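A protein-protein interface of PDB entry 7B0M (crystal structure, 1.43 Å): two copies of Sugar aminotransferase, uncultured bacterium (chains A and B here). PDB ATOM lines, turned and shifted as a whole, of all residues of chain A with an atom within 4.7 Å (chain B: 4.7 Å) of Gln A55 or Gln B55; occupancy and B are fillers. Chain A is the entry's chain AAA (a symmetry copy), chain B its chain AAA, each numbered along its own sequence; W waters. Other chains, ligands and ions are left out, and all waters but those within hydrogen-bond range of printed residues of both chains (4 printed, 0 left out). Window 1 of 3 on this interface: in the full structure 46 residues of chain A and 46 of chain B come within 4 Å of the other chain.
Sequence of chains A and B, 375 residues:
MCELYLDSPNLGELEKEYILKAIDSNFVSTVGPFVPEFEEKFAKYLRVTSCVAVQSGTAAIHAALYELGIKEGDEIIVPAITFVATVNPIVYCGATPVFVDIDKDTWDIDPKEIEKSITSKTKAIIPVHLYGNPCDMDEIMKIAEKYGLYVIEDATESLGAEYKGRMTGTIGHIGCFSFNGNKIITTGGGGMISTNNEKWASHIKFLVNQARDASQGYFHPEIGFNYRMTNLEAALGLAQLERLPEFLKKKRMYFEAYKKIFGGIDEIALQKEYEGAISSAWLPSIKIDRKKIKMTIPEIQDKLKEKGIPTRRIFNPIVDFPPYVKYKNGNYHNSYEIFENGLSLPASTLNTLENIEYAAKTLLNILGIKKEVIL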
ATOM      1  N   VAL A  54       3.034 -12.729  31.077  1.00  0.00           N
ATOM      2  CA  VAL A  54       3.170 -11.393  31.706  1.00  0.00           C
ATOM      3  C   VAL A  54       4.386 -10.684  31.154  1.00  0.00           C
ATOM      4  O   VAL A  54       5.134 -11.182  30.307  1.00  0.00           O
ATOM      5  CB  VAL A  54       3.162 -11.498  33.242  1.00  0.00           C
ATOM      6  CG1 VAL A  54       1.818 -12.014  33.752  1.00  0.00           C
ATOM      7  CG2 VAL A  54       4.320 -12.376  33.749  1.00  0.00           C
ATOM      8  N   GLN A  55       4.537  -9.395  31.600  1.00  0.00           N
ATOM      9  CA  GLN A  55       5.546  -8.500  30.962  1.00  0.00           C
ATOM     10  C   GLN A  55       6.955  -8.706  31.506  1.00  0.00           C
ATOM     11  O   GLN A  55       7.887  -8.255  30.817  1.00  0.00           O
ATOM     12  CB  GLN A  55       5.209  -7.003  31.081  1.00  0.00           C
ATOM     13  CG  GLN A  55       6.089  -6.086  30.204  1.00  0.00           C
ATOM     14  CD  GLN A  55       6.377  -6.597  28.803  1.00  0.00           C
ATOM     15  OE1 GLN A  55       5.431  -6.973  28.069  1.00  0.00           O
ATOM     16  NE2 GLN A  55       7.679  -6.578  28.428  1.00  0.00           N
ATOM     17  N   SER A  56       7.120  -9.418  32.619  1.00  0.00           N
ATOM     18  CA  SER A  56       8.490  -9.675  33.146  1.00  0.00           C
ATOM     19  C   SER A  56       8.404 -10.781  34.198  1.00  0.00           C
ATOM     20  O   SER A  56       7.328 -11.082  34.773  1.00  0.00           O
ATOM     21  CB  SER A  56       9.070  -8.422  33.778  1.00  0.00           C
ATOM     22  OG  SER A  56       8.416  -8.055  34.994  1.00  0.00           O
ATOM     23  N   ALA A  59       7.150  -9.108  37.343  1.00  0.00           N
ATOM     24  CA  ALA A  59       5.705  -9.009  37.359  1.00  0.00           C
ATOM     25  C   ALA A  59       5.070 -10.357  37.726  1.00  0.00           C
ATOM     26  O   ALA A  59       4.055 -10.363  38.435  1.00  0.00           O
ATOM     27  CB  ALA A  59       5.176  -8.511  36.051  1.00  0.00           C
ATOM     28  N   GLY A 189      11.569  -8.768  26.715  1.00  0.00           N
ATOM     29  CA  GLY A 189      11.092  -8.707  28.072  1.00  0.00           C
ATOM     30  C   GLY A 189       9.838  -9.530  28.167  1.00  0.00           C
ATOM     31  O   GLY A 189       9.035  -9.568  27.226  1.00  0.00           O
ATOM     32  N   GLY A 190       9.672 -10.254  29.251  1.00  0.00           N
ATOM     33  CA  GLY A 190       8.489 -11.072  29.443  1.00  0.00           C
ATOM     34  C   GLY A 190       8.616 -12.035  30.601  1.00  0.00           C
ATOM     35  O   GLY A 190       9.707 -12.152  31.222  1.00  0.00           O
ATOM     36  N   GLY A 191       7.503 -12.620  30.987  1.00  0.00           N
ATOM     37  CA  GLY A 191       7.567 -13.676  31.987  1.00  0.00           C
ATOM     38  C   GLY A 191       6.350 -14.550  31.899  1.00  0.00           C
ATOM     39  O   GLY A 191       5.474 -14.369  31.007  1.00  0.00           O
ATOM     40  N   TYR A 227       0.127  -5.759  33.374  1.00  0.00           N
ATOM     41  CA  TYR A 227       1.247  -6.740  33.419  1.00  0.00           C
ATOM     42  C   TYR A 227       1.139  -7.770  32.299  1.00  0.00           C
ATOM     43  O   TYR A 227       1.950  -8.728  32.275  1.00  0.00           O
ATOM     44  CB  TYR A 227       1.294  -7.405  34.779  1.00  0.00           C
ATOM     45  CG  TYR A 227       1.945  -6.681  35.919  1.00  0.00           C
ATOM     46  CD1 TYR A 227       2.860  -5.651  35.747  1.00  0.00           C
ATOM     47  CD2 TYR A 227       1.754  -7.134  37.182  1.00  0.00           C
ATOM     48  CE1 TYR A 227       3.480  -5.066  36.846  1.00  0.00           C
ATOM     49  CE2 TYR A 227       2.432  -6.622  38.274  1.00  0.00           C
ATOM     50  CZ  TYR A 227       3.255  -5.535  38.113  1.00  0.00           C
ATOM     51  OH  TYR A 227       3.972  -5.030  39.165  1.00  0.00           O
ATOM     52  N   ARG A 228       0.278  -7.619  31.304  1.00  0.00           N
ATOM     53  CA  ARG A 228       0.166  -8.666  30.260  1.00  0.00           C
ATOM     54  C   ARG A 228       1.365  -8.654  29.320  1.00  0.00           C
ATOM     55  O   ARG A 228       2.014  -7.622  29.074  1.00  0.00           O
ATOM     56  CB  ARG A 228      -1.120  -8.485  29.449  1.00  0.00           C
ATOM     57  CG  ARG A 228      -0.980  -7.552  28.269  1.00  0.00           C
ATOM     58  CD  ARG A 228      -1.416  -6.153  28.507  1.00  0.00           C
ATOM     59  NE  ARG A 228      -2.850  -6.010  28.823  1.00  0.00           N
ATOM     60  CZ  ARG A 228      -3.403  -4.811  29.020  1.00  0.00           C
ATOM     61  NH1 ARG A 228      -4.688  -4.694  29.374  1.00  0.00           N
ATOM     62  NH2 ARG A 228      -2.621  -3.728  28.871  1.00  0.00           N
ATOM     63  N   MET A 229       1.769  -9.830  28.880  1.00  0.00           N
ATOM     64  CA  MET A 229       2.668  -9.929  27.727  1.00  0.00           C
ATOM     65  C   MET A 229       1.928  -9.412  26.472  1.00  0.00           C
ATOM     66  O   MET A 229       0.703  -9.636  26.311  1.00  0.00           O
ATOM     67  CB  MET A 229       3.050 -11.416  27.487  1.00  0.00           C
ATOM     68  CG  MET A 229       4.074 -11.531  26.433  1.00  0.00           C
ATOM     69  SD  MET A 229       4.672 -13.248  26.211  1.00  0.00           S
ATOM     70  CE  MET A 229       5.736 -13.302  27.653  1.00  0.00           C
ATOM     71  N   THR A 230       2.696  -8.792  25.599  1.00  0.00           N
ATOM     72  CA  THR A 230       2.156  -8.391  24.284  1.00  0.00           C
ATOM     73  C   THR A 230       2.219  -9.515  23.271  1.00  0.00           C
ATOM     74  O   THR A 230       2.983 -10.457  23.422  1.00  0.00           O
ATOM     75  CB  THR A 230       2.878  -7.158  23.764  1.00  0.00           C
ATOM     76  OG1 THR A 230       4.171  -7.548  23.313  1.00  0.00           O
ATOM     77  CG2 THR A 230       2.954  -6.083  24.804  1.00  0.00           C
ATOM     78  N   GLU A 233       5.676  -9.894  21.756  1.00  0.00           N
ATOM     79  CA  GLU A 233       6.556 -10.697  22.629  1.00  0.00           C
ATOM     80  C   GLU A 233       6.198 -12.171  22.504  1.00  0.00           C
ATOM     81  O   GLU A 233       7.153 -12.972  22.394  1.00  0.00           O
ATOM     82  CB  GLU A 233       6.406 -10.226  24.068  1.00  0.00           C
ATOM     83  CG  GLU A 233       7.070  -8.859  24.210  1.00  0.00           C
ATOM     84  CD  GLU A 233       6.816  -8.139  25.501  1.00  0.00           C
ATOM     85  OE1 GLU A 233       7.657  -7.185  25.775  1.00  0.00           O
ATOM     86  OE2 GLU A 233       5.839  -8.461  26.230  1.00  0.00           O
ATOM     87  N   VAL B  54       9.565   3.405  28.996  1.00  0.00           N
ATOM     88  CA  VAL B  54       9.049   2.433  29.988  1.00  0.00           C
ATOM     89  C   VAL B  54       8.120   1.448  29.312  1.00  0.00           C
ATOM     90  O   VAL B  54       7.853   1.486  28.107  1.00  0.00           O
ATOM     91  CB  VAL B  54       8.413   3.151  31.193  1.00  0.00           C
ATOM     92  CG1 VAL B  54       9.456   3.954  31.967  1.00  0.00           C
ATOM     93  CG2 VAL B  54       7.239   4.045  30.756  1.00  0.00           C
ATOM     94  N   GLN B  55       7.672   0.443  30.132  1.00  0.00           N
ATOM     95  CA  GLN B  55       6.949  -0.725  29.550  1.00  0.00           C
ATOM     96  C   GLN B  55       5.469  -0.452  29.309  1.00  0.00           C
ATOM     97  O   GLN B  55       4.879  -1.230  28.538  1.00  0.00           O
ATOM     98  CB  GLN B  55       7.061  -2.006  30.396  1.00  0.00           C
ATOM     99  CG  GLN B  55       6.553  -3.279  29.684  1.00  0.00           C
ATOM    100  CD  GLN B  55       6.937  -3.410  28.220  1.00  0.00           C
ATOM    101  OE1 GLN B  55       8.135  -3.276  27.875  1.00  0.00           O
ATOM    102  NE2 GLN B  55       5.921  -3.703  27.372  1.00  0.00           N
ATOM    103  N   SER B  56       4.916   0.631  29.851  1.00  0.00           N
ATOM    104  CA  SER B  56       3.483   0.948  29.592  1.00  0.00           C
ATOM    105  C   SER B  56       3.219   2.388  30.032  1.00  0.00           C
ATOM    106  O   SER B  56       3.973   2.997  30.832  1.00  0.00           O
ATOM    107  CB  SER B  56       2.573   0.010  30.366  1.00  0.00           C
ATOM    108  OG  SER B  56       2.611   0.231  31.777  1.00  0.00           O
ATOM    109  N   ALA B  59       2.854   2.261  33.789  1.00  0.00           N
ATOM    110  CA  ALA B  59       4.139   2.315  34.456  1.00  0.00           C
ATOM    111  C   ALA B  59       4.683   3.749  34.475  1.00  0.00           C
ATOM    112  O   ALA B  59       5.297   4.139  35.478  1.00  0.00           O
ATOM    113  CB  ALA B  59       5.124   1.382  33.823  1.00  0.00           C
ATOM    114  N   GLY B 189       3.354  -2.776  23.446  1.00  0.00           N
ATOM    115  CA  GLY B 189       3.202  -2.236  24.772  1.00  0.00           C
ATOM    116  C   GLY B 189       4.369  -1.330  25.047  1.00  0.00           C
ATOM    117  O   GLY B 189       5.495  -1.600  24.611  1.00  0.00           O
ATOM    118  N   GLY B 190       4.127  -0.217  25.702  1.00  0.00           N
ATOM    119  CA  GLY B 190       5.189   0.718  26.028  1.00  0.00           C
ATOM    120  C   GLY B 190       4.674   2.050  26.522  1.00  0.00           C
ATOM    121  O   GLY B 190       3.440   2.305  26.514  1.00  0.00           O
ATOM    122  N   GLY B 191       5.568   2.844  27.069  1.00  0.00           N
ATOM    123  CA  GLY B 191       5.187   4.204  27.424  1.00  0.00           C
ATOM    124  C   GLY B 191       6.403   5.078  27.515  1.00  0.00           C
ATOM    125  O   GLY B 191       7.553   4.635  27.238  1.00  0.00           O
ATOM    126  N   TYR B 227      10.545  -1.725  34.914  1.00  0.00           N
ATOM    127  CA  TYR B 227       9.611  -0.922  34.077  1.00  0.00           C
ATOM    128  C   TYR B 227      10.281  -0.429  32.799  1.00  0.00           C
ATOM    129  O   TYR B 227       9.651   0.356  32.047  1.00  0.00           O
ATOM    130  CB  TYR B 227       9.054   0.230  34.889  1.00  0.00           C
ATOM    131  CG  TYR B 227       7.914  -0.028  35.829  1.00  0.00           C
ATOM    132  CD1 TYR B 227       7.066  -1.121  35.719  1.00  0.00           C
ATOM    133  CD2 TYR B 227       7.594   0.914  36.750  1.00  0.00           C
ATOM    134  CE1 TYR B 227       5.986  -1.266  36.582  1.00  0.00           C
ATOM    135  CE2 TYR B 227       6.471   0.827  37.553  1.00  0.00           C
ATOM    136  CZ  TYR B 227       5.695  -0.305  37.514  1.00  0.00           C
ATOM    137  OH  TYR B 227       4.555  -0.406  38.266  1.00  0.00           O
ATOM    138  N   ARG B 228      11.464  -0.887  32.420  1.00  0.00           N
ATOM    139  CA  ARG B 228      12.107  -0.348  31.198  1.00  0.00           C
ATOM    140  C   ARG B 228      11.426  -0.854  29.933  1.00  0.00           C
ATOM    141  O   ARG B 228      10.848  -1.953  29.876  1.00  0.00           O
ATOM    142  CB  ARG B 228      13.592  -0.719  31.160  1.00  0.00           C
ATOM    143  CG  ARG B 228      13.878  -2.059  30.524  1.00  0.00           C
ATOM    144  CD  ARG B 228      14.037  -3.192  31.468  1.00  0.00           C
ATOM    145  NE  ARG B 228      15.181  -3.059  32.391  1.00  0.00           N
ATOM    146  CZ  ARG B 228      15.482  -4.016  33.271  1.00  0.00           C
ATOM    147  NH1 ARG B 228      16.477  -3.857  34.150  1.00  0.00           N
ATOM    148  NH2 ARG B 228      14.737  -5.136  33.258  1.00  0.00           N
ATOM    149  N   MET B 229      11.360  -0.001  28.929  1.00  0.00           N
ATOM    150  CA  MET B 229      11.050  -0.464  27.573  1.00  0.00           C
ATOM    151  C   MET B 229      12.200  -1.372  27.081  1.00  0.00           C
ATOM    152  O   MET B 229      13.393  -1.118  27.379  1.00  0.00           O
ATOM    153  CB  MET B 229      10.949   0.755  26.614  1.00  0.00           C
ATOM    154  CG  MET B 229      10.485   0.334  25.279  1.00  0.00           C
ATOM    155  SD  MET B 229      10.204   1.749  24.150  1.00  0.00           S
ATOM    156  CE  MET B 229       8.639   2.282  24.844  1.00  0.00           C
ATOM    157  N   THR B 230      11.819  -2.363  26.299  1.00  0.00           N
ATOM    158  CA  THR B 230      12.826  -3.210  25.626  1.00  0.00           C
ATOM    159  C   THR B 230      13.306  -2.604  24.324  1.00  0.00           C
ATOM    160  O   THR B 230      12.644  -1.759  23.740  1.00  0.00           O
ATOM    161  CB  THR B 230      12.280  -4.609  25.398  1.00  0.00           C
ATOM    162  OG1 THR B 230      11.344  -4.561  24.326  1.00  0.00           O
ATOM    163  CG2 THR B 230      11.667  -5.173  26.644  1.00  0.00           C
ATOM    164  N   GLU B 233      10.873  -3.201  21.476  1.00  0.00           N
ATOM    165  CA  GLU B 233       9.785  -2.201  21.484  1.00  0.00           C
ATOM    166  C   GLU B 233      10.301  -0.877  20.937  1.00  0.00           C
ATOM    167  O   GLU B 233       9.564  -0.285  20.118  1.00  0.00           O
ATOM    168  CB  GLU B 233       9.265  -2.032  22.904  1.00  0.00           C
ATOM    169  CG  GLU B 233       8.477  -3.280  23.291  1.00  0.00           C
ATOM    170  CD  GLU B 233       8.089  -3.388  24.736  1.00  0.00           C
ATOM    171  OE1 GLU B 233       7.126  -4.224  24.987  1.00  0.00           O
ATOM    172  OE2 GLU B 233       8.690  -2.707  25.611  1.00  0.00           O
HETATM  173  O   HOH W   1       5.741  -2.836  39.712  1.00  0.00           O
HETATM  174  O   HOH W   2       5.690  -5.349  22.776  1.00  0.00           O
HETATM  175  O   HOH W   3       9.994  -6.922  24.138  1.00  0.00           O
HETATM  176  O   HOH W   4       2.521  -2.348  38.847  1.00  0.00           O
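The side-chain amide nitrogen of Gln A55 lies close to the side-chain amide oxygen of Gln B55 (3.4 Å).
OE1 of Glu B233 lies close to OE1 of Glu A233, 3.1 Å away.
NE2 of Gln B55 lies within hydrogen-bond range of O of Gly B189, at 3.5 Å.
The backbone NH (N) of Gln B55 is in hydrogen-bond range of the backbone carbonyl oxygen (O) of Tyr B227, 2.8 Å away.
The side-chain carboxylate (OE2) of Glu B233 lies close to the side-chain amide oxygen (OE1) of Gln B55 (2.4 Å).
The backbone carbonyl oxygen (O) of Gln A55 is in hydrogen-bond range of the backbone NH (N) of Gly A190.
The side-chain carboxylate of Glu A233 lies close to the side-chain amide oxygen of Gln A55, 2.4 Å away.
N of Glu A233 sits at hydrogen-bond distance from OG1 of Thr A230 (3.2 Å).
Among the printed residues, merely in contact across the chains: Gly A189 with Thr B230 and Thr A230 with Gly B189.
Printed residues of chain B within 4 Å of Gln A55: Gln B55 (2.9 Å).
Printed residues of chain B within 4 Å of Gly A189: Thr B230.
Printed residues of chain B within 4 Å of Glu A233: Glu B233.
Val B54 touches none of the printed residues of chain A.
Of the printed residues of chain A, Gln B55 touches Gln A55 (2.9 Å).
Of the printed residues of chain A, Gly B189 touches Thr A230 (3.6 Å).
Met B229 touches none of the printed residues of chain A.
Of the printed residues of chain A, Thr B230 touches Gly A189.
Printed residues of chain A within 4 Å of Glu B233: Glu A233 (3.1 Å).
The nearest printed residue of chain A that does not touch Gln B55 is Glu A233 (4.2 Å).
The nearest printed residue of chain A that does not touch Thr B230 is Glu A233 (4.6 Å).
Among the printed residues, 4 pairs touch across the chains.
Gln B55 touches its own counterpart, Gln A55.
Gly A189 touches Thr B230, and with the chains exchanged Thr A230 touches Gly B189.
Glu A233 touches its own counterpart, Glu B233.
12 positions are printed for both chains.
Of the 4 pairs that touch across the chains among the printed residues, 4 have their exchanged pair printed and touching as well.
Water W3 bridges the side-chain hydroxyl (OG1) of Thr B230 (2.7 Å) and the side-chain carboxylate (OE1) of Glu A233 (2.9 Å).
Water W2 bridges OG1 of Thr A230 and OE1 of Glu B233.
Water W1 lies within hydrogen-bond range of OH of Tyr A227 (2.9 Å) and OH of Tyr B227 (3.1 Å).
Water W4 lies within hydrogen-bond range of the side-chain hydroxyl of Tyr B227 and the side-chain hydroxyl of Tyr A227.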
